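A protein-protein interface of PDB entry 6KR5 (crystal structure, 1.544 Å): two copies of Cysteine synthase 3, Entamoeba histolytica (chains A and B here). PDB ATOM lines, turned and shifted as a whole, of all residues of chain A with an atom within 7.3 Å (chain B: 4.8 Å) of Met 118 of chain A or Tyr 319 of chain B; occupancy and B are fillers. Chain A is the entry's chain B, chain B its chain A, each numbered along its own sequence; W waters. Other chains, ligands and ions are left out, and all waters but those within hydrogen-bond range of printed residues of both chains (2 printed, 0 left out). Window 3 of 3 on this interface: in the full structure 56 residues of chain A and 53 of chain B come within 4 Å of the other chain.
No position is printed for both chains.
Met 118 of chain A touches just these residues of chain B: Leu 314 (3.3 Å) and Tyr 319 (3.8 Å).
Of chain A, only Met 118 and Ala 122 come within 4 Å of Tyr 319 of chain B.
Printed residues of chain A within 4 Å of Leu 314 of chain B: Glu 115 (3.7 Å), Met 118 (3.3 Å) and Ile 119 (3.9 Å).
Of the printed residues of chain A, Val 270 of chain B touches Ala 122 and Phe 123.
Printed residues of chain B within 4 Å of Phe 123 of chain A: Val 270.
Of the printed residues of chain A, Met 276 of chain B touches Ile 119.
Lys 320 of chain B touches none of the printed residues of chain A.
Asp 317 of chain B touches none of the printed residues of chain A.
The nearest residue of chain A that does not touch Tyr 319 of chain B is Ile 119 of chain A (6.3 Å).
The nearest printed residue of chain B that does not touch Ala 122 of chain A is Met 276 of chain B (4.3 Å).
The backbone carbonyl oxygen (O) of Met 276 of chain B lies within hydrogen-bond range of the backbone NH (N) of Gly 310 of chain B.
Water W1 lies within hydrogen-bond range of the backbone carbonyl oxygen of Thr 316 of chain B (2.6 Å), the backbone NH of Tyr 319 of chain B (2.9 Å), the side-chain sulfur of Met 118 of chain A (3.3 Å) and the backbone NH of Leu 318 of chain B (3.4 Å).
Water W2 bridges O of Leu 314 of chain B (3.3 Å) and SD of Met 118 of chain A (3.6 Å).
Among the printed residues, pairs that only touch across the chains: Glu 115 of chain A with Leu 314 of chain B, Met 118 of chain A with Tyr 319 of chain B, Ile 119 of chain A with Met 276 of chain B, Ile 119 of chain A with Leu 314 of chain B, Ala 122 of chain A with Val 270 of chain B, Ala 122 of chain A with Tyr 319 of chain B and Phe 123 of chain A with Val 270 of chain B.
The side-chain sulfur (SD) of Met 118 of chain A lies close to the backbone carbonyl oxygen (O) of Leu 314 of chain B (3.3 Å).
Hydrophobic or aromatic side chains of chain A that line the printed part of chain B: Met 118, Ile 119, Ala 122 and Phe 123.
Of the 12 printed residues of chain B, 4 touch a printed residue of chain A.
Hydrophobic or aromatic side chains of chain B within 4 Å of the printed part of chain A: Val 270, Met 276, Leu 314 and Tyr 319.
Among the printed residues, 8 pairs touch across the chains.
Among the printed residues, no Asp or Glu carboxylate lies within 4 Å of a Lys or Arg side-chain nitrogen of the other chain.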
ATOM      1  N   MET A 108     -20.527 -11.414 -34.302  1.00  0.00           N
ATOM      2  CA  MET A 108     -19.605 -10.374 -33.855  1.00  0.00           C
ATOM      3  C   MET A 108     -18.229 -11.007 -33.661  1.00  0.00           C
ATOM      4  O   MET A 108     -18.127 -12.216 -33.449  1.00  0.00           O
ATOM      5  CB  MET A 108     -20.089  -9.741 -32.543  1.00  0.00           C
ATOM      6  CG  MET A 108     -20.353 -10.779 -31.471  1.00  0.00           C
ATOM      7  SD  MET A 108     -21.291 -10.115 -30.095  1.00  0.00           S
ATOM      8  CE  MET A 108     -20.350  -8.622 -29.779  1.00  0.00           C
ATOM      9  N   SER A 113     -16.899  -5.984 -27.620  1.00  0.00           N
ATOM     10  CA  SER A 113     -17.869  -5.663 -26.571  1.00  0.00           C
ATOM     11  C   SER A 113     -18.299  -6.878 -25.764  1.00  0.00           C
ATOM     12  O   SER A 113     -19.445  -7.334 -25.862  1.00  0.00           O
ATOM     13  CB  SER A 113     -19.100  -4.975 -27.160  1.00  0.00           C
ATOM     14  OG  SER A 113     -19.807  -4.294 -26.137  1.00  0.00           O
ATOM     15  N   VAL A 114     -17.374  -7.400 -24.961  1.00  0.00           N
ATOM     16  CA  VAL A 114     -17.638  -8.600 -24.175  1.00  0.00           C
ATOM     17  C   VAL A 114     -18.770  -8.373 -23.181  1.00  0.00           C
ATOM     18  O   VAL A 114     -19.498  -9.311 -22.841  1.00  0.00           O
ATOM     19  CB  VAL A 114     -16.350  -9.077 -23.475  1.00  0.00           C
ATOM     20  CG1 VAL A 114     -15.375  -9.615 -24.510  1.00  0.00           C
ATOM     21  CG2 VAL A 114     -15.723  -7.941 -22.692  1.00  0.00           C
ATOM     22  N   GLU A 115     -18.959  -7.134 -22.718  1.00  0.00           N
ATOM     23  CA  GLU A 115     -20.093  -6.855 -21.839  1.00  0.00           C
ATOM     24  C   GLU A 115     -21.410  -6.982 -22.591  1.00  0.00           C
ATOM     25  O   GLU A 115     -22.374  -7.562 -22.074  1.00  0.00           O
ATOM     26  CB  GLU A 115     -19.960  -5.464 -21.218  1.00  0.00           C
ATOM     27  CG  GLU A 115     -18.701  -5.281 -20.400  1.00  0.00           C
ATOM     28  CD  GLU A 115     -18.553  -3.866 -19.877  1.00  0.00           C
ATOM     29  OE1 GLU A 115     -18.688  -2.918 -20.682  1.00  0.00           O
ATOM     30  OE2 GLU A 115     -18.300  -3.705 -18.663  1.00  0.00           O
ATOM     31  N   ARG A 116     -21.467  -6.466 -23.825  1.00  0.00           N
ATOM     32  CA  ARG A 116     -22.686  -6.613 -24.611  1.00  0.00           C
ATOM     33  C   ARG A 116     -22.923  -8.067 -24.982  1.00  0.00           C
ATOM     34  O   ARG A 116     -24.075  -8.507 -25.052  1.00  0.00           O
ATOM     35  CB  ARG A 116     -22.628  -5.746 -25.870  1.00  0.00           C
ATOM     36  CG  ARG A 116     -22.974  -4.296 -25.626  1.00  0.00           C
ATOM     37  CD  ARG A 116     -23.236  -3.612 -26.953  1.00  0.00           C
ATOM     38  NE  ARG A 116     -23.522  -2.188 -26.820  1.00  0.00           N
ATOM     39  CZ  ARG A 116     -22.586  -1.253 -26.681  1.00  0.00           C
ATOM     40  NH1 ARG A 116     -21.301  -1.595 -26.644  1.00  0.00           N
ATOM     41  NH2 ARG A 116     -22.932   0.019 -26.574  1.00  0.00           N
ATOM     42  N   GLN A 117     -21.842  -8.820 -25.230  1.00  0.00           N
ATOM     43  CA  GLN A 117     -21.951 -10.270 -25.391  1.00  0.00           C
ATOM     44  C   GLN A 117     -22.675 -10.893 -24.221  1.00  0.00           C
ATOM     45  O   GLN A 117     -23.553 -11.744 -24.392  1.00  0.00           O
ATOM     46  CB  GLN A 117     -20.572 -10.912 -25.507  1.00  0.00           C
ATOM     47  CG  GLN A 117     -19.929 -10.768 -26.833  1.00  0.00           C
ATOM     48  CD  GLN A 117     -18.646 -11.554 -26.938  1.00  0.00           C
ATOM     49  OE1 GLN A 117     -18.570 -12.706 -26.505  1.00  0.00           O
ATOM     50  NE2 GLN A 117     -17.617 -10.932 -27.513  1.00  0.00           N
ATOM     51  N   MET A 118     -22.277 -10.507 -23.007  1.00  0.00           N
ATOM     52  CA  MET A 118     -22.886 -11.075 -21.814  1.00  0.00           C
ATOM     53  C   MET A 118     -24.356 -10.683 -21.717  1.00  0.00           C
ATOM     54  O   MET A 118     -25.199 -11.512 -21.358  1.00  0.00           O
ATOM     55  CB  MET A 118     -22.098 -10.619 -20.588  1.00  0.00           C
ATOM     56  CG  MET A 118     -22.623 -11.108 -19.266  1.00  0.00           C
ATOM     57  SD  MET A 118     -21.484 -10.583 -17.959  1.00  0.00           S
ATOM     58  CE  MET A 118     -19.990 -11.438 -18.437  1.00  0.00           C
ATOM     59  N   ILE A 119     -24.684  -9.431 -22.041  1.00  0.00           N
ATOM     60  CA  ILE A 119     -26.087  -9.013 -22.015  1.00  0.00           C
ATOM     61  C   ILE A 119     -26.895  -9.832 -23.012  1.00  0.00           C
ATOM     62  O   ILE A 119     -27.964 -10.362 -22.688  1.00  0.00           O
ATOM     63  CB  ILE A 119     -26.223  -7.509 -22.307  1.00  0.00           C
ATOM     64  CG1 ILE A 119     -25.639  -6.651 -21.187  1.00  0.00           C
ATOM     65  CG2 ILE A 119     -27.691  -7.132 -22.529  1.00  0.00           C
ATOM     66  CD1 ILE A 119     -25.568  -5.190 -21.583  1.00  0.00           C
ATOM     67  N   MET A 120     -26.387  -9.964 -24.241  1.00  0.00           N
ATOM     68  CA  MET A 120     -27.137 -10.692 -25.261  1.00  0.00           C
ATOM     69  C   MET A 120     -27.259 -12.173 -24.917  1.00  0.00           C
ATOM     70  O   MET A 120     -28.346 -12.755 -25.029  1.00  0.00           O
ATOM     71  CB  MET A 120     -26.478 -10.477 -26.622  1.00  0.00           C
ATOM     72  CG  MET A 120     -26.657  -9.053 -27.127  1.00  0.00           C
ATOM     73  SD  MET A 120     -25.900  -8.830 -28.733  1.00  0.00           S
ATOM     74  CE  MET A 120     -24.240  -9.249 -28.281  1.00  0.00           C
ATOM     75  N   LYS A 121     -26.169 -12.792 -24.453  1.00  0.00           N
ATOM     76  CA  LYS A 121     -26.249 -14.185 -24.016  1.00  0.00           C
ATOM     77  C   LYS A 121     -27.257 -14.359 -22.879  1.00  0.00           C
ATOM     78  O   LYS A 121     -27.972 -15.368 -22.829  1.00  0.00           O
ATOM     79  CB  LYS A 121     -24.868 -14.684 -23.590  1.00  0.00           C
ATOM     80  N   ALA A 122     -27.346 -13.375 -21.969  1.00  0.00           N
ATOM     81  CA  ALA A 122     -28.302 -13.488 -20.867  1.00  0.00           C
ATOM     82  C   ALA A 122     -29.739 -13.523 -21.371  1.00  0.00           C
ATOM     83  O   ALA A 122     -30.589 -14.220 -20.794  1.00  0.00           O
ATOM     84  CB  ALA A 122     -28.113 -12.339 -19.873  1.00  0.00           C
ATOM     85  N   PHE A 123     -30.023 -12.799 -22.463  1.00  0.00           N
ATOM     86  CA  PHE A 123     -31.330 -12.829 -23.103  1.00  0.00           C
ATOM     87  C   PHE A 123     -31.561 -14.088 -23.931  1.00  0.00           C
ATOM     88  O   PHE A 123     -32.633 -14.229 -24.530  1.00  0.00           O
ATOM     89  CB  PHE A 123     -31.504 -11.588 -23.981  1.00  0.00           C
ATOM     90  CG  PHE A 123     -31.994 -10.375 -23.232  1.00  0.00           C
ATOM     91  CD1 PHE A 123     -33.355 -10.126 -23.103  1.00  0.00           C
ATOM     92  CD2 PHE A 123     -31.097  -9.465 -22.679  1.00  0.00           C
ATOM     93  CE1 PHE A 123     -33.810  -8.990 -22.422  1.00  0.00           C
ATOM     94  CE2 PHE A 123     -31.551  -8.332 -22.005  1.00  0.00           C
ATOM     95  CZ  PHE A 123     -32.906  -8.099 -21.881  1.00  0.00           C
ATOM     96  N   GLY A 124     -30.605 -15.008 -23.966  1.00  0.00           N
ATOM     97  CA  GLY A 124     -30.771 -16.240 -24.707  1.00  0.00           C
ATOM     98  C   GLY A 124     -30.263 -16.202 -26.128  1.00  0.00           C
ATOM     99  O   GLY A 124     -30.551 -17.131 -26.895  1.00  0.00           O
ATOM    100  N   LEU A 127     -24.751 -16.482 -29.777  1.00  0.00           N
ATOM    101  CA  LEU A 127     -23.646 -15.678 -30.272  1.00  0.00           C
ATOM    102  C   LEU A 127     -22.811 -16.478 -31.257  1.00  0.00           C
ATOM    103  O   LEU A 127     -22.375 -17.598 -30.958  1.00  0.00           O
ATOM    104  CB  LEU A 127     -22.770 -15.186 -29.120  1.00  0.00           C
ATOM    105  CG  LEU A 127     -23.473 -14.211 -28.194  1.00  0.00           C
ATOM    106  CD1 LEU A 127     -22.451 -13.611 -27.245  1.00  0.00           C
ATOM    107  CD2 LEU A 127     -24.178 -13.118 -28.978  1.00  0.00           C
ATOM    108  N   ARG B 267     -31.195 -15.020 -13.738  1.00  0.00           N
ATOM    109  CA  ARG B 267     -30.928 -15.518 -15.083  1.00  0.00           C
ATOM    110  C   ARG B 267     -32.211 -15.978 -15.756  1.00  0.00           C
ATOM    111  O   ARG B 267     -32.395 -15.763 -16.959  1.00  0.00           O
ATOM    112  CB  ARG B 267     -29.905 -16.656 -15.040  1.00  0.00           C
ATOM    113  CG  ARG B 267     -28.523 -16.176 -14.699  1.00  0.00           C
ATOM    114  CD  ARG B 267     -27.466 -17.262 -14.863  1.00  0.00           C
ATOM    115  NE  ARG B 267     -27.655 -18.413 -13.987  1.00  0.00           N
ATOM    116  CZ  ARG B 267     -27.068 -18.556 -12.798  1.00  0.00           C
ATOM    117  NH1 ARG B 267     -26.285 -17.592 -12.303  1.00  0.00           N
ATOM    118  NH2 ARG B 267     -27.280 -19.654 -12.087  1.00  0.00           N
ATOM    119  N   VAL B 270     -34.524 -12.896 -16.992  1.00  0.00           N
ATOM    120  CA  VAL B 270     -34.133 -12.234 -18.233  1.00  0.00           C
ATOM    121  C   VAL B 270     -34.332 -13.161 -19.435  1.00  0.00           C
ATOM    122  O   VAL B 270     -34.769 -12.706 -20.498  1.00  0.00           O
ATOM    123  CB  VAL B 270     -32.702 -11.663 -18.108  1.00  0.00           C
ATOM    124  CG1 VAL B 270     -31.652 -12.744 -17.878  1.00  0.00           C
ATOM    125  CG2 VAL B 270     -32.353 -10.801 -19.323  1.00  0.00           C
ATOM    126  N   MET B 276     -34.054  -7.694 -17.467  1.00  0.00           N
ATOM    127  CA  MET B 276     -32.698  -7.933 -16.970  1.00  0.00           C
ATOM    128  C   MET B 276     -32.543  -7.298 -15.595  1.00  0.00           C
ATOM    129  O   MET B 276     -31.945  -6.236 -15.417  1.00  0.00           O
ATOM    130  CB  MET B 276     -31.653  -7.415 -17.944  1.00  0.00           C
ATOM    131  CG  MET B 276     -30.258  -7.802 -17.514  1.00  0.00           C
ATOM    132  SD  MET B 276     -29.058  -7.366 -18.777  1.00  0.00           S
ATOM    133  CE  MET B 276     -27.653  -8.365 -18.255  1.00  0.00           C
ATOM    134  N   CYS B 277     -33.064  -8.000 -14.601  1.00  0.00           N
ATOM    135  CA  CYS B 277     -33.062  -7.514 -13.232  1.00  0.00           C
ATOM    136  C   CYS B 277     -31.764  -7.885 -12.509  1.00  0.00           C
ATOM    137  O   CYS B 277     -31.014  -8.768 -12.925  1.00  0.00           O
ATOM    138  CB  CYS B 277     -34.274  -8.090 -12.509  1.00  0.00           C
ATOM    139  SG  CYS B 277     -34.289  -9.875 -12.306  1.00  0.00           S
ATOM    140  N   GLY B 310     -29.496  -5.889 -14.042  1.00  0.00           N
ATOM    141  CA  GLY B 310     -28.364  -6.795 -14.103  1.00  0.00           C
ATOM    142  C   GLY B 310     -27.141  -6.236 -14.807  1.00  0.00           C
ATOM    143  O   GLY B 310     -26.034  -6.725 -14.562  1.00  0.00           O
ATOM    144  N   LEU B 314     -22.296  -6.949 -14.544  1.00  0.00           N
ATOM    145  CA  LEU B 314     -21.605  -7.708 -15.584  1.00  0.00           C
ATOM    146  C   LEU B 314     -20.209  -8.131 -15.144  1.00  0.00           C
ATOM    147  O   LEU B 314     -19.688  -9.147 -15.623  1.00  0.00           O
ATOM    148  CB  LEU B 314     -21.541  -6.887 -16.870  1.00  0.00           C
ATOM    149  CG  LEU B 314     -22.892  -6.524 -17.491  1.00  0.00           C
ATOM    150  CD1 LEU B 314     -22.699  -5.779 -18.813  1.00  0.00           C
ATOM    151  CD2 LEU B 314     -23.749  -7.762 -17.689  1.00  0.00           C
ATOM    152  N   THR B 316     -19.493  -9.266 -12.234  1.00  0.00           N
ATOM    153  CA  THR B 316     -19.650 -10.343 -11.271  1.00  0.00           C
ATOM    154  C   THR B 316     -19.858 -11.671 -11.989  1.00  0.00           C
ATOM    155  O   THR B 316     -19.867 -11.753 -13.220  1.00  0.00           O
ATOM    156  CB  THR B 316     -20.842 -10.088 -10.353  1.00  0.00           C
ATOM    157  OG1 THR B 316     -22.044 -10.429 -11.064  1.00  0.00           O
ATOM    158  CG2 THR B 316     -20.893  -8.634  -9.926  1.00  0.00           C
ATOM    159  N   ASP B 317     -20.085 -12.722 -11.202  1.00  0.00           N
ATOM    160  CA  ASP B 317     -20.382 -14.037 -11.749  1.00  0.00           C
ATOM    161  C   ASP B 317     -21.873 -14.277 -11.974  1.00  0.00           C
ATOM    162  O   ASP B 317     -22.278 -15.426 -12.179  1.00  0.00           O
ATOM    163  CB  ASP B 317     -19.803 -15.127 -10.849  1.00  0.00           C
ATOM    164  CG  ASP B 317     -18.448 -15.594 -11.324  1.00  0.00           C
ATOM    165  OD1 ASP B 317     -17.667 -14.749 -11.819  1.00  0.00           O
ATOM    166  OD2 ASP B 317     -18.175 -16.810 -11.217  1.00  0.00           O
ATOM    167  N   LEU B 318     -22.688 -13.221 -11.970  1.00  0.00           N
ATOM    168  CA  LEU B 318     -24.133 -13.394 -12.104  1.00  0.00           C
ATOM    169  C   LEU B 318     -24.492 -14.195 -13.350  1.00  0.00           C
ATOM    170  O   LEU B 318     -25.334 -15.098 -13.293  1.00  0.00           O
ATOM    171  CB  LEU B 318     -24.822 -12.033 -12.136  1.00  0.00           C
ATOM    172  CG  LEU B 318     -26.339 -12.065 -12.296  1.00  0.00           C
ATOM    173  CD1 LEU B 318     -26.991 -13.006 -11.262  1.00  0.00           C
ATOM    174  CD2 LEU B 318     -26.876 -10.652 -12.190  1.00  0.00           C
ATOM    175  N   TYR B 319     -23.872 -13.872 -14.487  1.00  0.00           N
ATOM    176  CA  TYR B 319     -24.200 -14.506 -15.760  1.00  0.00           C
ATOM    177  C   TYR B 319     -23.124 -15.488 -16.215  1.00  0.00           C
ATOM    178  O   TYR B 319     -23.112 -15.891 -17.383  1.00  0.00           O
ATOM    179  CB  TYR B 319     -24.452 -13.443 -16.832  1.00  0.00           C
ATOM    180  CG  TYR B 319     -25.572 -12.488 -16.458  1.00  0.00           C
ATOM    181  CD1 TYR B 319     -26.902 -12.909 -16.452  1.00  0.00           C
ATOM    182  CD2 TYR B 319     -25.292 -11.184 -16.070  1.00  0.00           C
ATOM    183  CE1 TYR B 319     -27.929 -12.049 -16.097  1.00  0.00           C
ATOM    184  CE2 TYR B 319     -26.312 -10.310 -15.715  1.00  0.00           C
ATOM    185  CZ  TYR B 319     -27.626 -10.752 -15.718  1.00  0.00           C
ATOM    186  OH  TYR B 319     -28.644  -9.886 -15.360  1.00  0.00           O
ATOM    187  N   LYS B 320     -22.230 -15.895 -15.311  1.00  0.00           N
ATOM    188  CA  LYS B 320     -21.229 -16.904 -15.651  1.00  0.00           C
ATOM    189  C   LYS B 320     -21.876 -18.271 -15.856  1.00  0.00           C
ATOM    190  O   LYS B 320     -21.799 -18.853 -16.945  1.00  0.00           O
ATOM    191  CB  LYS B 320     -20.160 -16.967 -14.555  1.00  0.00           C
ATOM    192  N   THR B 321     -22.520 -18.799 -14.816  1.00  0.00           N
ATOM    193  CA  THR B 321     -23.156 -20.108 -14.915  1.00  0.00           C
ATOM    194  C   THR B 321     -24.295 -20.067 -15.926  1.00  0.00           C
ATOM    195  O   THR B 321     -25.059 -19.101 -15.986  1.00  0.00           O
ATOM    196  CB  THR B 321     -23.681 -20.549 -13.548  1.00  0.00           C
ATOM    197  OG1 THR B 321     -22.587 -20.675 -12.629  1.00  0.00           O
ATOM    198  CG2 THR B 321     -24.413 -21.884 -13.643  1.00  0.00           C
HETATM  199  O   HOH W   1     -21.720 -11.979 -15.020  1.00  0.00           O
HETATM  200  O   HOH W   2     -18.635  -8.480 -18.680  1.00  0.00           O
